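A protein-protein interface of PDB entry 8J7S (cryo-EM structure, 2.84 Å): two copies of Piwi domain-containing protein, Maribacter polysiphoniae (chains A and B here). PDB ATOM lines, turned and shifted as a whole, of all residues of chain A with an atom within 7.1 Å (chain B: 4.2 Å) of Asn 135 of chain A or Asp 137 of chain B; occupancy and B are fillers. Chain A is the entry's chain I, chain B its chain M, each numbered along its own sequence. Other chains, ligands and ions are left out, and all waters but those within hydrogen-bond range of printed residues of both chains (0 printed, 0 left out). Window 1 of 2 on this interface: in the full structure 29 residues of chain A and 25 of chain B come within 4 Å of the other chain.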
ATOM      1  N   ILE A  39      23.624 -26.743 -24.390  1.00  0.00           N
ATOM      2  CA  ILE A  39      23.221 -25.369 -24.119  1.00  0.00           C
ATOM      3  C   ILE A  39      24.250 -24.751 -23.183  1.00  0.00           C
ATOM      4  O   ILE A  39      24.511 -25.286 -22.099  1.00  0.00           O
ATOM      5  CB  ILE A  39      21.814 -25.290 -23.508  1.00  0.00           C
ATOM      6  CG1 ILE A  39      20.788 -25.939 -24.436  1.00  0.00           C
ATOM      7  CG2 ILE A  39      21.435 -23.849 -23.229  1.00  0.00           C
ATOM      8  CD1 ILE A  39      19.386 -25.929 -23.889  1.00  0.00           C
ATOM      9  N   LYS A  40      24.827 -23.627 -23.599  1.00  0.00           N
ATOM     10  CA  LYS A  40      25.762 -22.874 -22.768  1.00  0.00           C
ATOM     11  C   LYS A  40      24.969 -21.807 -22.024  1.00  0.00           C
ATOM     12  O   LYS A  40      24.631 -20.764 -22.585  1.00  0.00           O
ATOM     13  CB  LYS A  40      26.867 -22.261 -23.620  1.00  0.00           C
ATOM     14  CG  LYS A  40      27.980 -23.228 -23.991  1.00  0.00           C
ATOM     15  CD  LYS A  40      28.382 -23.067 -25.448  1.00  0.00           C
ATOM     16  CE  LYS A  40      29.731 -23.707 -25.724  1.00  0.00           C
ATOM     17  NZ  LYS A  40      29.890 -24.078 -27.157  1.00  0.00           N
ATOM     18  N   SER A  41      24.672 -22.070 -20.756  1.00  0.00           N
ATOM     19  CA  SER A  41      23.827 -21.180 -19.972  1.00  0.00           C
ATOM     20  C   SER A  41      24.639 -20.029 -19.392  1.00  0.00           C
ATOM     21  O   SER A  41      25.703 -20.239 -18.802  1.00  0.00           O
ATOM     22  CB  SER A  41      23.145 -21.953 -18.845  1.00  0.00           C
ATOM     23  OG  SER A  41      22.579 -23.155 -19.327  1.00  0.00           O
ATOM     24  N   GLY A  42      24.127 -18.812 -19.555  1.00  0.00           N
ATOM     25  CA  GLY A  42      24.717 -17.649 -18.928  1.00  0.00           C
ATOM     26  C   GLY A  42      23.744 -16.981 -17.982  1.00  0.00           C
ATOM     27  O   GLY A  42      22.698 -16.487 -18.407  1.00  0.00           O
ATOM     28  N   GLY A  90      28.060 -25.899 -17.849  1.00  0.00           N
ATOM     29  CA  GLY A  90      28.077 -24.811 -18.802  1.00  0.00           C
ATOM     30  C   GLY A  90      27.574 -23.485 -18.276  1.00  0.00           C
ATOM     31  O   GLY A  90      27.404 -22.550 -19.066  1.00  0.00           O
ATOM     32  N   THR A  92      27.630 -19.882 -16.651  1.00  0.00           N
ATOM     33  CA  THR A  92      28.566 -18.768 -16.549  1.00  0.00           C
ATOM     34  C   THR A  92      27.877 -17.652 -15.777  1.00  0.00           C
ATOM     35  O   THR A  92      26.914 -17.058 -16.269  1.00  0.00           O
ATOM     36  CB  THR A  92      29.000 -18.295 -17.934  1.00  0.00           C
ATOM     37  OG1 THR A  92      29.809 -19.306 -18.543  1.00  0.00           O
ATOM     38  CG2 THR A  92      29.790 -17.003 -17.833  1.00  0.00           C
ATOM     39  N   ALA A 128      29.437  -8.889 -21.043  1.00  0.00           N
ATOM     40  CA  ALA A 128      29.807 -10.293 -21.164  1.00  0.00           C
ATOM     41  C   ALA A 128      29.671 -10.808 -22.592  1.00  0.00           C
ATOM     42  O   ALA A 128      30.249 -11.847 -22.920  1.00  0.00           O
ATOM     43  CB  ALA A 128      28.962 -11.143 -20.218  1.00  0.00           C
ATOM     44  N   ASN A 129      28.917 -10.110 -23.442  1.00  0.00           N
ATOM     45  CA  ASN A 129      28.807 -10.503 -24.842  1.00  0.00           C
ATOM     46  C   ASN A 129      29.968  -9.973 -25.675  1.00  0.00           C
ATOM     47  O   ASN A 129      30.417 -10.638 -26.614  1.00  0.00           O
ATOM     48  CB  ASN A 129      27.478 -10.008 -25.416  1.00  0.00           C
ATOM     49  CG  ASN A 129      27.331 -10.308 -26.895  1.00  0.00           C
ATOM     50  OD1 ASN A 129      27.650 -11.403 -27.354  1.00  0.00           O
ATOM     51  ND2 ASN A 129      26.845  -9.331 -27.650  1.00  0.00           N
ATOM     52  N   GLU A 132      34.233 -10.732 -23.478  1.00  0.00           N
ATOM     53  CA  GLU A 132      34.567 -12.020 -22.896  1.00  0.00           C
ATOM     54  C   GLU A 132      34.695 -13.033 -24.022  1.00  0.00           C
ATOM     55  O   GLU A 132      34.144 -12.852 -25.110  1.00  0.00           O
ATOM     56  CB  GLU A 132      33.524 -12.474 -21.870  1.00  0.00           C
ATOM     57  CG  GLU A 132      33.700 -11.832 -20.508  1.00  0.00           C
ATOM     58  CD  GLU A 132      33.103 -12.659 -19.392  1.00  0.00           C
ATOM     59  OE1 GLU A 132      32.572 -13.751 -19.679  1.00  0.00           O
ATOM     60  OE2 GLU A 132      33.167 -12.218 -18.226  1.00  0.00           O
ATOM     61  N   ASP A 133      35.440 -14.102 -23.753  1.00  0.00           N
ATOM     62  CA  ASP A 133      35.707 -15.113 -24.766  1.00  0.00           C
ATOM     63  C   ASP A 133      34.819 -16.341 -24.640  1.00  0.00           C
ATOM     64  O   ASP A 133      34.629 -17.051 -25.633  1.00  0.00           O
ATOM     65  CB  ASP A 133      37.177 -15.542 -24.709  1.00  0.00           C
ATOM     66  CG  ASP A 133      38.068 -14.678 -25.582  1.00  0.00           C
ATOM     67  OD1 ASP A 133      37.939 -14.746 -26.823  1.00  0.00           O
ATOM     68  OD2 ASP A 133      38.895 -13.925 -25.026  1.00  0.00           O
ATOM     69  N   GLU A 134      34.273 -16.604 -23.457  1.00  0.00           N
ATOM     70  CA  GLU A 134      33.370 -17.731 -23.282  1.00  0.00           C
ATOM     71  C   GLU A 134      32.070 -17.500 -24.044  1.00  0.00           C
ATOM     72  O   GLU A 134      31.531 -16.391 -24.067  1.00  0.00           O
ATOM     73  CB  GLU A 134      33.085 -17.948 -21.798  1.00  0.00           C
ATOM     74  CG  GLU A 134      32.042 -19.007 -21.521  1.00  0.00           C
ATOM     75  CD  GLU A 134      30.701 -18.411 -21.168  1.00  0.00           C
ATOM     76  OE1 GLU A 134      30.619 -17.173 -21.040  1.00  0.00           O
ATOM     77  OE2 GLU A 134      29.728 -19.181 -21.017  1.00  0.00           O
ATOM     78  N   ASN A 135      31.564 -18.561 -24.667  1.00  0.00           N
ATOM     79  CA  ASN A 135      30.356 -18.486 -25.478  1.00  0.00           C
ATOM     80  C   ASN A 135      29.131 -18.818 -24.635  1.00  0.00           C
ATOM     81  O   ASN A 135      29.154 -19.757 -23.834  1.00  0.00           O
ATOM     82  CB  ASN A 135      30.451 -19.440 -26.669  1.00  0.00           C
ATOM     83  CG  ASN A 135      29.781 -18.890 -27.906  1.00  0.00           C
ATOM     84  OD1 ASN A 135      29.199 -17.808 -27.880  1.00  0.00           O
ATOM     85  ND2 ASN A 135      29.862 -19.632 -29.002  1.00  0.00           N
ATOM     86  N   VAL A 136      28.067 -18.040 -24.816  1.00  0.00           N
ATOM     87  CA  VAL A 136      26.793 -18.255 -24.140  1.00  0.00           C
ATOM     88  C   VAL A 136      25.712 -18.395 -25.202  1.00  0.00           C
ATOM     89  O   VAL A 136      25.650 -17.591 -26.138  1.00  0.00           O
ATOM     90  CB  VAL A 136      26.459 -17.109 -23.171  1.00  0.00           C
ATOM     91  CG1 VAL A 136      25.154 -17.383 -22.465  1.00  0.00           C
ATOM     92  CG2 VAL A 136      27.572 -16.929 -22.163  1.00  0.00           C
ATOM     93  N   ASP A 137      24.870 -19.418 -25.058  1.00  0.00           N
ATOM     94  CA  ASP A 137      23.773 -19.644 -25.994  1.00  0.00           C
ATOM     95  C   ASP A 137      22.493 -18.947 -25.538  1.00  0.00           C
ATOM     96  O   ASP A 137      21.872 -18.210 -26.308  1.00  0.00           O
ATOM     97  CB  ASP A 137      23.537 -21.148 -26.171  1.00  0.00           C
ATOM     98  N   VAL A 138      22.089 -19.173 -24.290  1.00  0.00           N
ATOM     99  CA  VAL A 138      20.887 -18.572 -23.724  1.00  0.00           C
ATOM    100  C   VAL A 138      21.268 -17.864 -22.432  1.00  0.00           C
ATOM    101  O   VAL A 138      21.882 -18.468 -21.547  1.00  0.00           O
ATOM    102  CB  VAL A 138      19.787 -19.618 -23.458  1.00  0.00           C
ATOM    103  CG1 VAL A 138      18.487 -18.937 -23.085  1.00  0.00           C
ATOM    104  CG2 VAL A 138      19.590 -20.499 -24.670  1.00  0.00           C
ATOM    105  N   TRP A 139      20.895 -16.591 -22.321  1.00  0.00           N
ATOM    106  CA  TRP A 139      21.172 -15.798 -21.129  1.00  0.00           C
ATOM    107  C   TRP A 139      19.957 -15.848 -20.212  1.00  0.00           C
ATOM    108  O   TRP A 139      18.904 -15.294 -20.535  1.00  0.00           O
ATOM    109  CB  TRP A 139      21.515 -14.359 -21.504  1.00  0.00           C
ATOM    110  CG  TRP A 139      22.964 -14.144 -21.805  1.00  0.00           C
ATOM    111  CD1 TRP A 139      23.546 -14.099 -23.035  1.00  0.00           C
ATOM    112  CD2 TRP A 139      24.018 -13.950 -20.857  1.00  0.00           C
ATOM    113  NE1 TRP A 139      24.895 -13.884 -22.914  1.00  0.00           N
ATOM    114  CE2 TRP A 139      25.210 -13.792 -21.585  1.00  0.00           C
ATOM    115  CE3 TRP A 139      24.069 -13.895 -19.461  1.00  0.00           C
ATOM    116  CZ2 TRP A 139      26.436 -13.582 -20.968  1.00  0.00           C
ATOM    117  CZ3 TRP A 139      25.288 -13.688 -18.852  1.00  0.00           C
ATOM    118  CH2 TRP A 139      26.454 -13.533 -19.602  1.00  0.00           C
ATOM    119  N   GLY B  38      29.909 -28.732 -29.006  1.00  0.00           N
ATOM    120  CA  GLY B  38      30.064 -28.894 -30.437  1.00  0.00           C
ATOM    121  C   GLY B  38      30.204 -27.541 -31.093  1.00  0.00           C
ATOM    122  O   GLY B  38      30.087 -26.494 -30.447  1.00  0.00           O
ATOM    123  N   LYS B  40      28.660 -25.385 -34.255  1.00  0.00           N
ATOM    124  CA  LYS B  40      27.625 -25.211 -35.265  1.00  0.00           C
ATOM    125  C   LYS B  40      28.132 -24.221 -36.304  1.00  0.00           C
ATOM    126  O   LYS B  40      28.360 -23.049 -35.990  1.00  0.00           O
ATOM    127  CB  LYS B  40      26.325 -24.719 -34.634  1.00  0.00           C
ATOM    128  CG  LYS B  40      25.928 -25.468 -33.373  1.00  0.00           C
ATOM    129  CD  LYS B  40      24.498 -25.972 -33.453  1.00  0.00           C
ATOM    130  CE  LYS B  40      24.433 -27.335 -34.122  1.00  0.00           C
ATOM    131  NZ  LYS B  40      23.194 -28.082 -33.767  1.00  0.00           N
ATOM    132  N   ASN B 135      21.084 -21.473 -34.450  1.00  0.00           N
ATOM    133  CA  ASN B 135      22.133 -20.816 -33.680  1.00  0.00           C
ATOM    134  C   ASN B 135      23.486 -21.222 -34.247  1.00  0.00           C
ATOM    135  O   ASN B 135      23.866 -22.396 -34.175  1.00  0.00           O
ATOM    136  CB  ASN B 135      22.039 -21.186 -32.202  1.00  0.00           C
ATOM    137  CG  ASN B 135      23.042 -20.442 -31.354  1.00  0.00           C
ATOM    138  OD1 ASN B 135      23.567 -19.407 -31.761  1.00  0.00           O
ATOM    139  ND2 ASN B 135      23.318 -20.965 -30.169  1.00  0.00           N
ATOM    140  N   VAL B 136      24.214 -20.254 -34.796  1.00  0.00           N
ATOM    141  CA  VAL B 136      25.503 -20.490 -35.436  1.00  0.00           C
ATOM    142  C   VAL B 136      26.593 -19.889 -34.562  1.00  0.00           C
ATOM    143  O   VAL B 136      26.511 -18.716 -34.174  1.00  0.00           O
ATOM    144  CB  VAL B 136      25.543 -19.896 -36.855  1.00  0.00           C
ATOM    145  CG1 VAL B 136      26.935 -20.003 -37.436  1.00  0.00           C
ATOM    146  CG2 VAL B 136      24.538 -20.599 -37.746  1.00  0.00           C
ATOM    147  N   ASP B 137      27.611 -20.691 -34.249  1.00  0.00           N
ATOM    148  CA  ASP B 137      28.714 -20.225 -33.414  1.00  0.00           C
ATOM    149  C   ASP B 137      29.738 -19.445 -34.231  1.00  0.00           C
ATOM    150  O   ASP B 137      29.988 -18.264 -33.970  1.00  0.00           O
ATOM    151  CB  ASP B 137      29.378 -21.414 -32.715  1.00  0.00           C
ATOM    152  CG  ASP B 137      28.639 -21.837 -31.463  1.00  0.00           C
ATOM    153  OD1 ASP B 137      27.440 -21.513 -31.343  1.00  0.00           O
ATOM    154  OD2 ASP B 137      29.257 -22.494 -30.599  1.00  0.00           O
ATOM    155  N   VAL B 138      30.337 -20.092 -35.225  1.00  0.00           N
ATOM    156  CA  VAL B 138      31.338 -19.478 -36.087  1.00  0.00           C
ATOM    157  C   VAL B 138      30.830 -19.521 -37.518  1.00  0.00           C
ATOM    158  O   VAL B 138      30.299 -20.543 -37.965  1.00  0.00           O
ATOM    159  CB  VAL B 138      32.705 -20.189 -35.972  1.00  0.00           C
ATOM    160  CG1 VAL B 138      33.773 -19.430 -36.742  1.00  0.00           C
ATOM    161  CG2 VAL B 138      33.106 -20.340 -34.521  1.00  0.00           C
ATOM    162  N   PRO B 220      31.556 -13.975 -34.394  1.00  0.00           N
ATOM    163  CA  PRO B 220      32.854 -14.610 -34.673  1.00  0.00           C
ATOM    164  C   PRO B 220      32.849 -15.263 -36.045  1.00  0.00           C
ATOM    165  O   PRO B 220      32.006 -16.106 -36.345  1.00  0.00           O
ATOM    166  CB  PRO B 220      32.988 -15.647 -33.553  1.00  0.00           C
ATOM    167  CG  PRO B 220      32.064 -15.182 -32.486  1.00  0.00           C
ATOM    168  CD  PRO B 220      30.921 -14.526 -33.188  1.00  0.00           C
ATOM    169  N   ALA B 264      35.099 -20.324 -31.248  1.00  0.00           N
ATOM    170  CA  ALA B 264      33.814 -20.834 -30.795  1.00  0.00           C
ATOM    171  C   ALA B 264      33.705 -20.880 -29.277  1.00  0.00           C
ATOM    172  O   ALA B 264      32.826 -21.566 -28.746  1.00  0.00           O
ATOM    173  CB  ALA B 264      33.557 -22.221 -31.385  1.00  0.00           C
ATOM    174  N   GLY B 265      34.582 -20.177 -28.569  1.00  0.00           N
ATOM    175  CA  GLY B 265      34.498 -20.076 -27.128  1.00  0.00           C
ATOM    176  C   GLY B 265      35.333 -21.058 -26.338  1.00  0.00           C
ATOM    177  O   GLY B 265      35.132 -21.168 -25.124  1.00  0.00           O
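Lys 40 of chain A touches Asp 137 of chain B, but with the chains exchanged Asp 137 of chain A does not touch Lys 40 of chain B (8.7 Å). Asn 135 of chain A touches Asp 137 of chain B, but with the chains exchanged Asp 137 of chain A does not touch Asn 135 of chain B (4.01 Å). Positions printed for both chains: 40, 135, 136, 137 and 138. Of the 4 pairs that touch across the chains among the printed residues, none has its exchanged pair printed and touching as well.
O of Lys 40 of chain A is in hydrogen-bond range of N of Asp 137 of chain A, 2.8 Å away. O of Lys 40 of chain A lies within hydrogen-bond range of N of Val 138 of chain A. The backbone carbonyl oxygen (O) of Lys 40 of chain B lies within hydrogen-bond range of the backbone NH (N) of Asp 137 of chain B, 3.0 Å away.
Ala 128 of chain A touches none of the printed residues of chain B. Of the printed residues of chain B, Asp 133 of chain A touches Gly 265 (3.4 Å). Asn 135 of chain A touches just these residues of chain B: Asp 137 and Ala 264. Lys 40 of chain B touches none of the printed residues of chain A. Printed residues of chain A within 4 Å of Ala 264 of chain B: Asn 135 (3.5 Å). The nearest residue of chain A that does not touch Asp 137 of chain B is Asp 137 of chain A (6.5 Å).
NZ of Lys 40 of chain A lies within salt-bridge range of OD2 of Asp 137 of chain B (3.8 Å). ND2 of Asn 135 of chain A lies within hydrogen-bond range of OD2 of Asp 137 of chain B (3.3 Å).
CA of Gly 265 of chain B touches O of Asp 133 of chain A, at 3.4 Å. ND2 of Asn 135 of chain A touches O of Ala 264 of chain B, at 3.5 Å.
Of the 16 printed residues of chain A, 3 touch a printed residue of chain B. Along chain B the printed residues that touch a printed residue of chain A span positions 137 to 265. Among the printed residues, Asp or Glu carboxylates within 4 Å of a Lys or Arg side-chain nitrogen of the other chain: Lys 40 of chain A with Asp 137 of chain B.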
